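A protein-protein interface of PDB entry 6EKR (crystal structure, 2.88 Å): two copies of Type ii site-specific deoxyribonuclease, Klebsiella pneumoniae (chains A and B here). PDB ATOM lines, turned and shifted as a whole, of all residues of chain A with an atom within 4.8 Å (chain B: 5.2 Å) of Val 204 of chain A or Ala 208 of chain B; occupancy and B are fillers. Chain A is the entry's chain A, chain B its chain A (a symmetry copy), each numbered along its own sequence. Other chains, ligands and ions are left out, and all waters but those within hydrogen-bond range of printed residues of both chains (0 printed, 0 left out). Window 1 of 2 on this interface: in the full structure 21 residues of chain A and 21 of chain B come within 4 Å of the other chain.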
ATOM      1  N   GLU A 201      10.538   4.253 -31.872  1.00  0.00           N
ATOM      2  CA  GLU A 201       9.383   4.579 -31.042  1.00  0.00           C
ATOM      3  C   GLU A 201       9.446   5.985 -30.449  1.00  0.00           C
ATOM      4  O   GLU A 201       8.457   6.486 -29.925  1.00  0.00           O
ATOM      5  CB  GLU A 201       9.219   3.551 -29.923  1.00  0.00           C
ATOM      6  CG  GLU A 201      10.369   3.528 -28.935  1.00  0.00           C
ATOM      7  CD  GLU A 201      11.610   2.886 -29.506  1.00  0.00           C
ATOM      8  OE1 GLU A 201      11.490   1.809 -30.121  1.00  0.00           O
ATOM      9  OE2 GLU A 201      12.707   3.452 -29.331  1.00  0.00           O
ATOM     10  N   ARG A 202      10.612   6.613 -30.529  1.00  0.00           N
ATOM     11  CA  ARG A 202      10.801   7.979 -30.024  1.00  0.00           C
ATOM     12  C   ARG A 202      10.232   9.043 -30.972  1.00  0.00           C
ATOM     13  O   ARG A 202      10.607  10.212 -30.897  1.00  0.00           O
ATOM     14  CB  ARG A 202      12.284   8.267 -29.755  1.00  0.00           C
ATOM     15  CG  ARG A 202      13.043   7.164 -29.045  1.00  0.00           C
ATOM     16  CD  ARG A 202      14.501   7.558 -28.713  1.00  0.00           C
ATOM     17  NE  ARG A 202      15.298   8.148 -29.812  1.00  0.00           N
ATOM     18  CZ  ARG A 202      15.718   7.509 -30.912  1.00  0.00           C
ATOM     19  NH1 ARG A 202      15.406   6.229 -31.137  1.00  0.00           N
ATOM     20  NH2 ARG A 202      16.448   8.169 -31.806  1.00  0.00           N
ATOM     21  N   ILE A 203       9.332   8.630 -31.860  1.00  0.00           N
ATOM     22  CA  ILE A 203       8.722   9.534 -32.836  1.00  0.00           C
ATOM     23  C   ILE A 203       7.699  10.470 -32.183  1.00  0.00           C
ATOM     24  O   ILE A 203       7.523  11.608 -32.633  1.00  0.00           O
ATOM     25  CB  ILE A 203       8.109   8.761 -34.061  1.00  0.00           C
ATOM     26  CG1 ILE A 203       7.423   9.710 -35.059  1.00  0.00           C
ATOM     27  CG2 ILE A 203       7.151   7.662 -33.615  1.00  0.00           C
ATOM     28  CD1 ILE A 203       8.374  10.616 -35.833  1.00  0.00           C
ATOM     29  N   VAL A 204       7.045   9.999 -31.119  1.00  0.00           N
ATOM     30  CA  VAL A 204       6.093  10.819 -30.367  1.00  0.00           C
ATOM     31  C   VAL A 204       6.783  11.980 -29.648  1.00  0.00           C
ATOM     32  O   VAL A 204       6.189  13.036 -29.456  1.00  0.00           O
ATOM     33  CB  VAL A 204       5.258   9.968 -29.360  1.00  0.00           C
ATOM     34  CG1 VAL A 204       6.167   9.125 -28.448  1.00  0.00           C
ATOM     35  CG2 VAL A 204       4.297  10.844 -28.542  1.00  0.00           C
ATOM     36  N   GLN A 205       8.044  11.779 -29.288  1.00  0.00           N
ATOM     37  CA  GLN A 205       8.775  12.696 -28.421  1.00  0.00           C
ATOM     38  C   GLN A 205       8.837  14.175 -28.908  1.00  0.00           C
ATOM     39  O   GLN A 205       8.569  15.097 -28.125  1.00  0.00           O
ATOM     40  CB  GLN A 205      10.162  12.118 -28.108  1.00  0.00           C
ATOM     41  CG  GLN A 205      10.625  12.336 -26.673  1.00  0.00           C
ATOM     42  CD  GLN A 205       9.817  11.527 -25.630  1.00  0.00           C
ATOM     43  OE1 GLN A 205      10.006  10.308 -25.468  1.00  0.00           O
ATOM     44  NE2 GLN A 205       8.922  12.221 -24.911  1.00  0.00           N
ATOM     45  N   PRO A 206       9.185  14.408 -30.191  1.00  0.00           N
ATOM     46  CA  PRO A 206       9.137  15.784 -30.693  1.00  0.00           C
ATOM     47  C   PRO A 206       7.734  16.390 -30.741  1.00  0.00           C
ATOM     48  O   PRO A 206       7.589  17.597 -30.558  1.00  0.00           O
ATOM     49  CB  PRO A 206       9.706  15.670 -32.112  1.00  0.00           C
ATOM     50  CG  PRO A 206       9.554  14.249 -32.479  1.00  0.00           C
ATOM     51  CD  PRO A 206       9.668  13.469 -31.217  1.00  0.00           C
ATOM     52  N   PHE A 207       6.721  15.564 -30.990  1.00  0.00           N
ATOM     53  CA  PHE A 207       5.341  16.030 -31.060  1.00  0.00           C
ATOM     54  C   PHE A 207       4.873  16.448 -29.684  1.00  0.00           C
ATOM     55  O   PHE A 207       4.429  17.566 -29.504  1.00  0.00           O
ATOM     56  CB  PHE A 207       4.411  14.959 -31.651  1.00  0.00           C
ATOM     57  CG  PHE A 207       4.566  14.760 -33.137  1.00  0.00           C
ATOM     58  CD1 PHE A 207       3.907  15.595 -34.036  1.00  0.00           C
ATOM     59  CD2 PHE A 207       5.372  13.737 -33.634  1.00  0.00           C
ATOM     60  CE1 PHE A 207       4.056  15.417 -35.417  1.00  0.00           C
ATOM     61  CE2 PHE A 207       5.528  13.550 -35.006  1.00  0.00           C
ATOM     62  CZ  PHE A 207       4.868  14.388 -35.902  1.00  0.00           C
ATOM     63  N   ALA A 208       4.999  15.550 -28.712  1.00  0.00           N
ATOM     64  CA  ALA A 208       4.652  15.840 -27.325  1.00  0.00           C
ATOM     65  C   ALA A 208       5.346  17.103 -26.814  1.00  0.00           C
ATOM     66  O   ALA A 208       4.717  17.949 -26.163  1.00  0.00           O
ATOM     67  CB  ALA A 208       4.996  14.678 -26.450  1.00  0.00           C
ATOM     68  N   TYR A 253      -0.483  12.244 -35.130  1.00  0.00           N
ATOM     69  CA  TYR A 253       0.324  13.172 -34.367  1.00  0.00           C
ATOM     70  C   TYR A 253       0.256  14.604 -34.900  1.00  0.00           C
ATOM     71  O   TYR A 253       0.012  15.523 -34.129  1.00  0.00           O
ATOM     72  CB  TYR A 253       1.766  12.679 -34.239  1.00  0.00           C
ATOM     73  CG  TYR A 253       1.957  11.490 -33.296  1.00  0.00           C
ATOM     74  CD1 TYR A 253       0.919  11.015 -32.493  1.00  0.00           C
ATOM     75  CD2 TYR A 253       3.196  10.860 -33.197  1.00  0.00           C
ATOM     76  CE1 TYR A 253       1.107   9.937 -31.643  1.00  0.00           C
ATOM     77  CE2 TYR A 253       3.398   9.788 -32.344  1.00  0.00           C
ATOM     78  CZ  TYR A 253       2.355   9.331 -31.569  1.00  0.00           C
ATOM     79  OH  TYR A 253       2.578   8.260 -30.727  1.00  0.00           O
ATOM     80  N   LEU A 257      -2.215  15.758 -32.081  1.00  0.00           N
ATOM     81  CA  LEU A 257      -1.281  15.976 -30.973  1.00  0.00           C
ATOM     82  C   LEU A 257      -0.576  17.327 -31.044  1.00  0.00           C
ATOM     83  O   LEU A 257      -0.587  18.091 -30.070  1.00  0.00           O
ATOM     84  CB  LEU A 257      -0.251  14.847 -30.874  1.00  0.00           C
ATOM     85  CG  LEU A 257       0.818  14.919 -29.775  1.00  0.00           C
ATOM     86  CD1 LEU A 257       0.196  14.990 -28.392  1.00  0.00           C
ATOM     87  CD2 LEU A 257       1.730  13.719 -29.868  1.00  0.00           C
ATOM     88  N   VAL B 204       5.310   8.804 -21.503  1.00  0.00           N
ATOM     89  CA  VAL B 204       4.645   9.822 -22.318  1.00  0.00           C
ATOM     90  C   VAL B 204       3.431   9.257 -23.059  1.00  0.00           C
ATOM     91  O   VAL B 204       2.466   9.972 -23.311  1.00  0.00           O
ATOM     92  CB  VAL B 204       5.629  10.503 -23.320  1.00  0.00           C
ATOM     93  CG1 VAL B 204       6.381   9.460 -24.167  1.00  0.00           C
ATOM     94  CG2 VAL B 204       4.911  11.535 -24.204  1.00  0.00           C
ATOM     95  N   GLN B 205       3.481   7.968 -23.366  1.00  0.00           N
ATOM     96  CA  GLN B 205       2.509   7.325 -24.243  1.00  0.00           C
ATOM     97  C   GLN B 205       1.018   7.469 -23.813  1.00  0.00           C
ATOM     98  O   GLN B 205       0.165   7.821 -24.640  1.00  0.00           O
ATOM     99  CB  GLN B 205       2.916   5.865 -24.486  1.00  0.00           C
ATOM    100  CG  GLN B 205       2.690   5.377 -25.912  1.00  0.00           C
ATOM    101  CD  GLN B 205       3.630   6.036 -26.950  1.00  0.00           C
ATOM    102  OE1 GLN B 205       4.820   5.688 -27.058  1.00  0.00           O
ATOM    103  NE2 GLN B 205       3.081   6.982 -27.725  1.00  0.00           N
ATOM    104  N   PRO B 206       0.698   7.204 -22.528  1.00  0.00           N
ATOM    105  CA  PRO B 206      -0.677   7.444 -22.082  1.00  0.00           C
ATOM    106  C   PRO B 206      -1.100   8.914 -22.106  1.00  0.00           C
ATOM    107  O   PRO B 206      -2.271   9.202 -22.341  1.00  0.00           O
ATOM    108  CB  PRO B 206      -0.685   6.922 -20.641  1.00  0.00           C
ATOM    109  CG  PRO B 206       0.731   6.907 -20.225  1.00  0.00           C
ATOM    110  CD  PRO B 206       1.533   6.646 -21.451  1.00  0.00           C
ATOM    111  N   PHE B 207      -0.160   9.823 -21.860  1.00  0.00           N
ATOM    112  CA  PHE B 207      -0.448  11.252 -21.855  1.00  0.00           C
ATOM    113  C   PHE B 207      -0.755  11.716 -23.262  1.00  0.00           C
ATOM    114  O   PHE B 207      -1.802  12.290 -23.499  1.00  0.00           O
ATOM    115  CB  PHE B 207       0.712  12.062 -21.255  1.00  0.00           C
ATOM    116  CG  PHE B 207       0.838  11.941 -19.758  1.00  0.00           C
ATOM    117  CD1 PHE B 207       0.064  12.734 -18.916  1.00  0.00           C
ATOM    118  CD2 PHE B 207       1.732  11.032 -19.194  1.00  0.00           C
ATOM    119  CE1 PHE B 207       0.174  12.619 -17.524  1.00  0.00           C
ATOM    120  CE2 PHE B 207       1.851  10.908 -17.811  1.00  0.00           C
ATOM    121  CZ  PHE B 207       1.074  11.702 -16.972  1.00  0.00           C
ATOM    122  N   ALA B 208       0.151  11.439 -24.193  1.00  0.00           N
ATOM    123  CA  ALA B 208      -0.045  11.766 -25.601  1.00  0.00           C
ATOM    124  C   ALA B 208      -1.367  11.218 -26.137  1.00  0.00           C
ATOM    125  O   ALA B 208      -2.104  11.923 -26.841  1.00  0.00           O
ATOM    126  CB  ALA B 208       1.093  11.244 -26.418  1.00  0.00           C
ATOM    127  N   GLN B 209      -1.673   9.969 -25.797  1.00  0.00           N
ATOM    128  CA  GLN B 209      -2.916   9.340 -26.231  1.00  0.00           C
ATOM    129  C   GLN B 209      -4.148  10.074 -25.696  1.00  0.00           C
ATOM    130  O   GLN B 209      -5.129  10.249 -26.422  1.00  0.00           O
ATOM    131  CB  GLN B 209      -2.938   7.879 -25.813  1.00  0.00           C
ATOM    132  CG  GLN B 209      -4.104   7.109 -26.356  1.00  0.00           C
ATOM    133  CD  GLN B 209      -4.106   5.668 -25.900  1.00  0.00           C
ATOM    134  OE1 GLN B 209      -4.336   4.755 -26.702  1.00  0.00           O
ATOM    135  NE2 GLN B 209      -3.842   5.447 -24.607  1.00  0.00           N
ATOM    136  N   GLN B 210      -4.087  10.503 -24.433  1.00  0.00           N
ATOM    137  CA  GLN B 210      -5.189  11.230 -23.801  1.00  0.00           C
ATOM    138  C   GLN B 210      -5.457  12.546 -24.529  1.00  0.00           C
ATOM    139  O   GLN B 210      -6.607  12.861 -24.872  1.00  0.00           O
ATOM    140  CB  GLN B 210      -4.891  11.474 -22.319  1.00  0.00           C
ATOM    141  CG  GLN B 210      -6.006  12.135 -21.516  1.00  0.00           C
ATOM    142  CD  GLN B 210      -7.395  11.577 -21.806  1.00  0.00           C
ATOM    143  OE1 GLN B 210      -8.292  12.327 -22.173  1.00  0.00           O
ATOM    144  NE2 GLN B 210      -7.576  10.265 -21.650  1.00  0.00           N
ATOM    145  N   ARG B 211      -4.378  13.291 -24.772  1.00  0.00           N
ATOM    146  CA  ARG B 211      -4.401  14.502 -25.571  1.00  0.00           C
ATOM    147  C   ARG B 211      -5.096  14.273 -26.909  1.00  0.00           C
ATOM    148  O   ARG B 211      -6.029  15.005 -27.267  1.00  0.00           O
ATOM    149  CB  ARG B 211      -2.976  14.991 -25.799  1.00  0.00           C
ATOM    150  CG  ARG B 211      -2.819  16.041 -26.883  1.00  0.00           C
ATOM    151  CD  ARG B 211      -3.314  17.396 -26.439  1.00  0.00           C
ATOM    152  NE  ARG B 211      -4.766  17.485 -26.524  1.00  0.00           N
ATOM    153  CZ  ARG B 211      -5.468  18.599 -26.330  1.00  0.00           C
ATOM    154  NH1 ARG B 211      -4.836  19.738 -26.046  1.00  0.00           N
ATOM    155  NH2 ARG B 211      -6.797  18.572 -26.430  1.00  0.00           N
ATOM    156  N   ILE B 212      -4.651  13.250 -27.638  1.00  0.00           N
ATOM    157  CA  ILE B 212      -5.194  12.954 -28.959  1.00  0.00           C
ATOM    158  C   ILE B 212      -6.691  12.667 -28.896  1.00  0.00           C
ATOM    159  O   ILE B 212      -7.447  13.189 -29.706  1.00  0.00           O
ATOM    160  CB  ILE B 212      -4.408  11.822 -29.665  1.00  0.00           C
ATOM    161  CG1 ILE B 212      -3.045  12.348 -30.122  1.00  0.00           C
ATOM    162  CG2 ILE B 212      -5.184  11.263 -30.866  1.00  0.00           C
ATOM    163  CD1 ILE B 212      -1.959  11.296 -30.154  1.00  0.00           C
ATOM    164  N   LEU B 213      -7.119  11.876 -27.916  1.00  0.00           N
ATOM    165  CA  LEU B 213      -8.542  11.555 -27.758  1.00  0.00           C
ATOM    166  C   LEU B 213      -9.399  12.770 -27.386  1.00  0.00           C
ATOM    167  O   LEU B 213     -10.560  12.864 -27.791  1.00  0.00           O
ATOM    168  CB  LEU B 213      -8.735  10.454 -26.723  1.00  0.00           C
ATOM    169  CG  LEU B 213      -8.110   9.096 -26.986  1.00  0.00           C
ATOM    170  CD1 LEU B 213      -7.917   8.399 -25.657  1.00  0.00           C
ATOM    171  CD2 LEU B 213      -8.964   8.270 -27.907  1.00  0.00           C
ATOM    172  N   LEU B 257       0.750  18.747 -21.084  1.00  0.00           N
ATOM    173  CA  LEU B 257       0.453  17.806 -22.166  1.00  0.00           C
ATOM    174  C   LEU B 257      -0.978  17.281 -22.124  1.00  0.00           C
ATOM    175  O   LEU B 257      -1.701  17.350 -23.127  1.00  0.00           O
ATOM    176  CB  LEU B 257       1.444  16.639 -22.186  1.00  0.00           C
ATOM    177  CG  LEU B 257       1.274  15.546 -23.250  1.00  0.00           C
ATOM    178  CD1 LEU B 257       1.330  16.118 -24.655  1.00  0.00           C
ATOM    179  CD2 LEU B 257       2.344  14.494 -23.080  1.00  0.00           C
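Val 204 of chain A touches two residues of chain B. Of the printed residues of chain B, Tyr 253 of chain A touches Gln 205 and Ile 212. Of the printed residues of chain B, Gln 205 of chain A touches Val 204. Of the printed residues of chain A, Ile 212 of chain B touches Tyr 253 and Leu 257. Gln 209 of chain B touches none of the printed residues of chain A. The nearest residue of chain A that does not touch Ala 208 of chain B is Leu 257 of chain A (4.1 Å).
Hydrophobic or aromatic side chains of chain A within 4 Å of the printed part of chain B: Val 204, Ala 208, Tyr 253 and Leu 257. Of the 11 printed residues of chain B, 5 touch a printed residue of chain A. Printed residues of chain B that touch a printed residue of chain A: Val 204, Gln 205, Ala 208, Arg 211 and Ile 212. Hydrophobic or aromatic side chains of chain B within 4 Å of the printed part of chain A: Val 204, Ala 208 and Ile 212. Among the printed residues, no Asp or Glu carboxylate lies within 4 Å of a Lys or Arg side-chain nitrogen of the other chain.
CG1 of Val 204 of chain A touches NE2 of Gln 205 of chain B, 3.8 Å away. CB of Ala 208 of chain B touches CG2 of Val 204 of chain A, at 3.9 Å. Val 204 of chain B touches Gln 205 of chain A. Ala 208 of chain A touches Val 204 of chain B. CE1 of Tyr 253 of chain A touches CD1 of Ile 212 of chain B, at 3.7 Å. Leu 257 of chain A touches Arg 211 of chain B. Leu 257 of chain A touches Ile 212 of chain B (CB to CG1, 3.8 Å).
The side-chain amide nitrogen (NE2) of Gln 205 of chain B sits at hydrogen-bond distance from the side-chain hydroxyl (OH) of Tyr 253 of chain A (3.3 Å).
Val 204 of chain A touches Gln 205 of chain B, and with the chains exchanged Gln 205 of chain A touches Val 204 of chain B. Val 204 of chain A touches Ala 208 of chain B, and with the chains exchanged Ala 208 of chain A touches Val 204 of chain B. Positions printed for both chains: 204, 205, 206, 207, 208 and 257. Of the 8 pairs that touch across the chains among the printed residues, 4 have their exchanged pair printed and touching as well.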
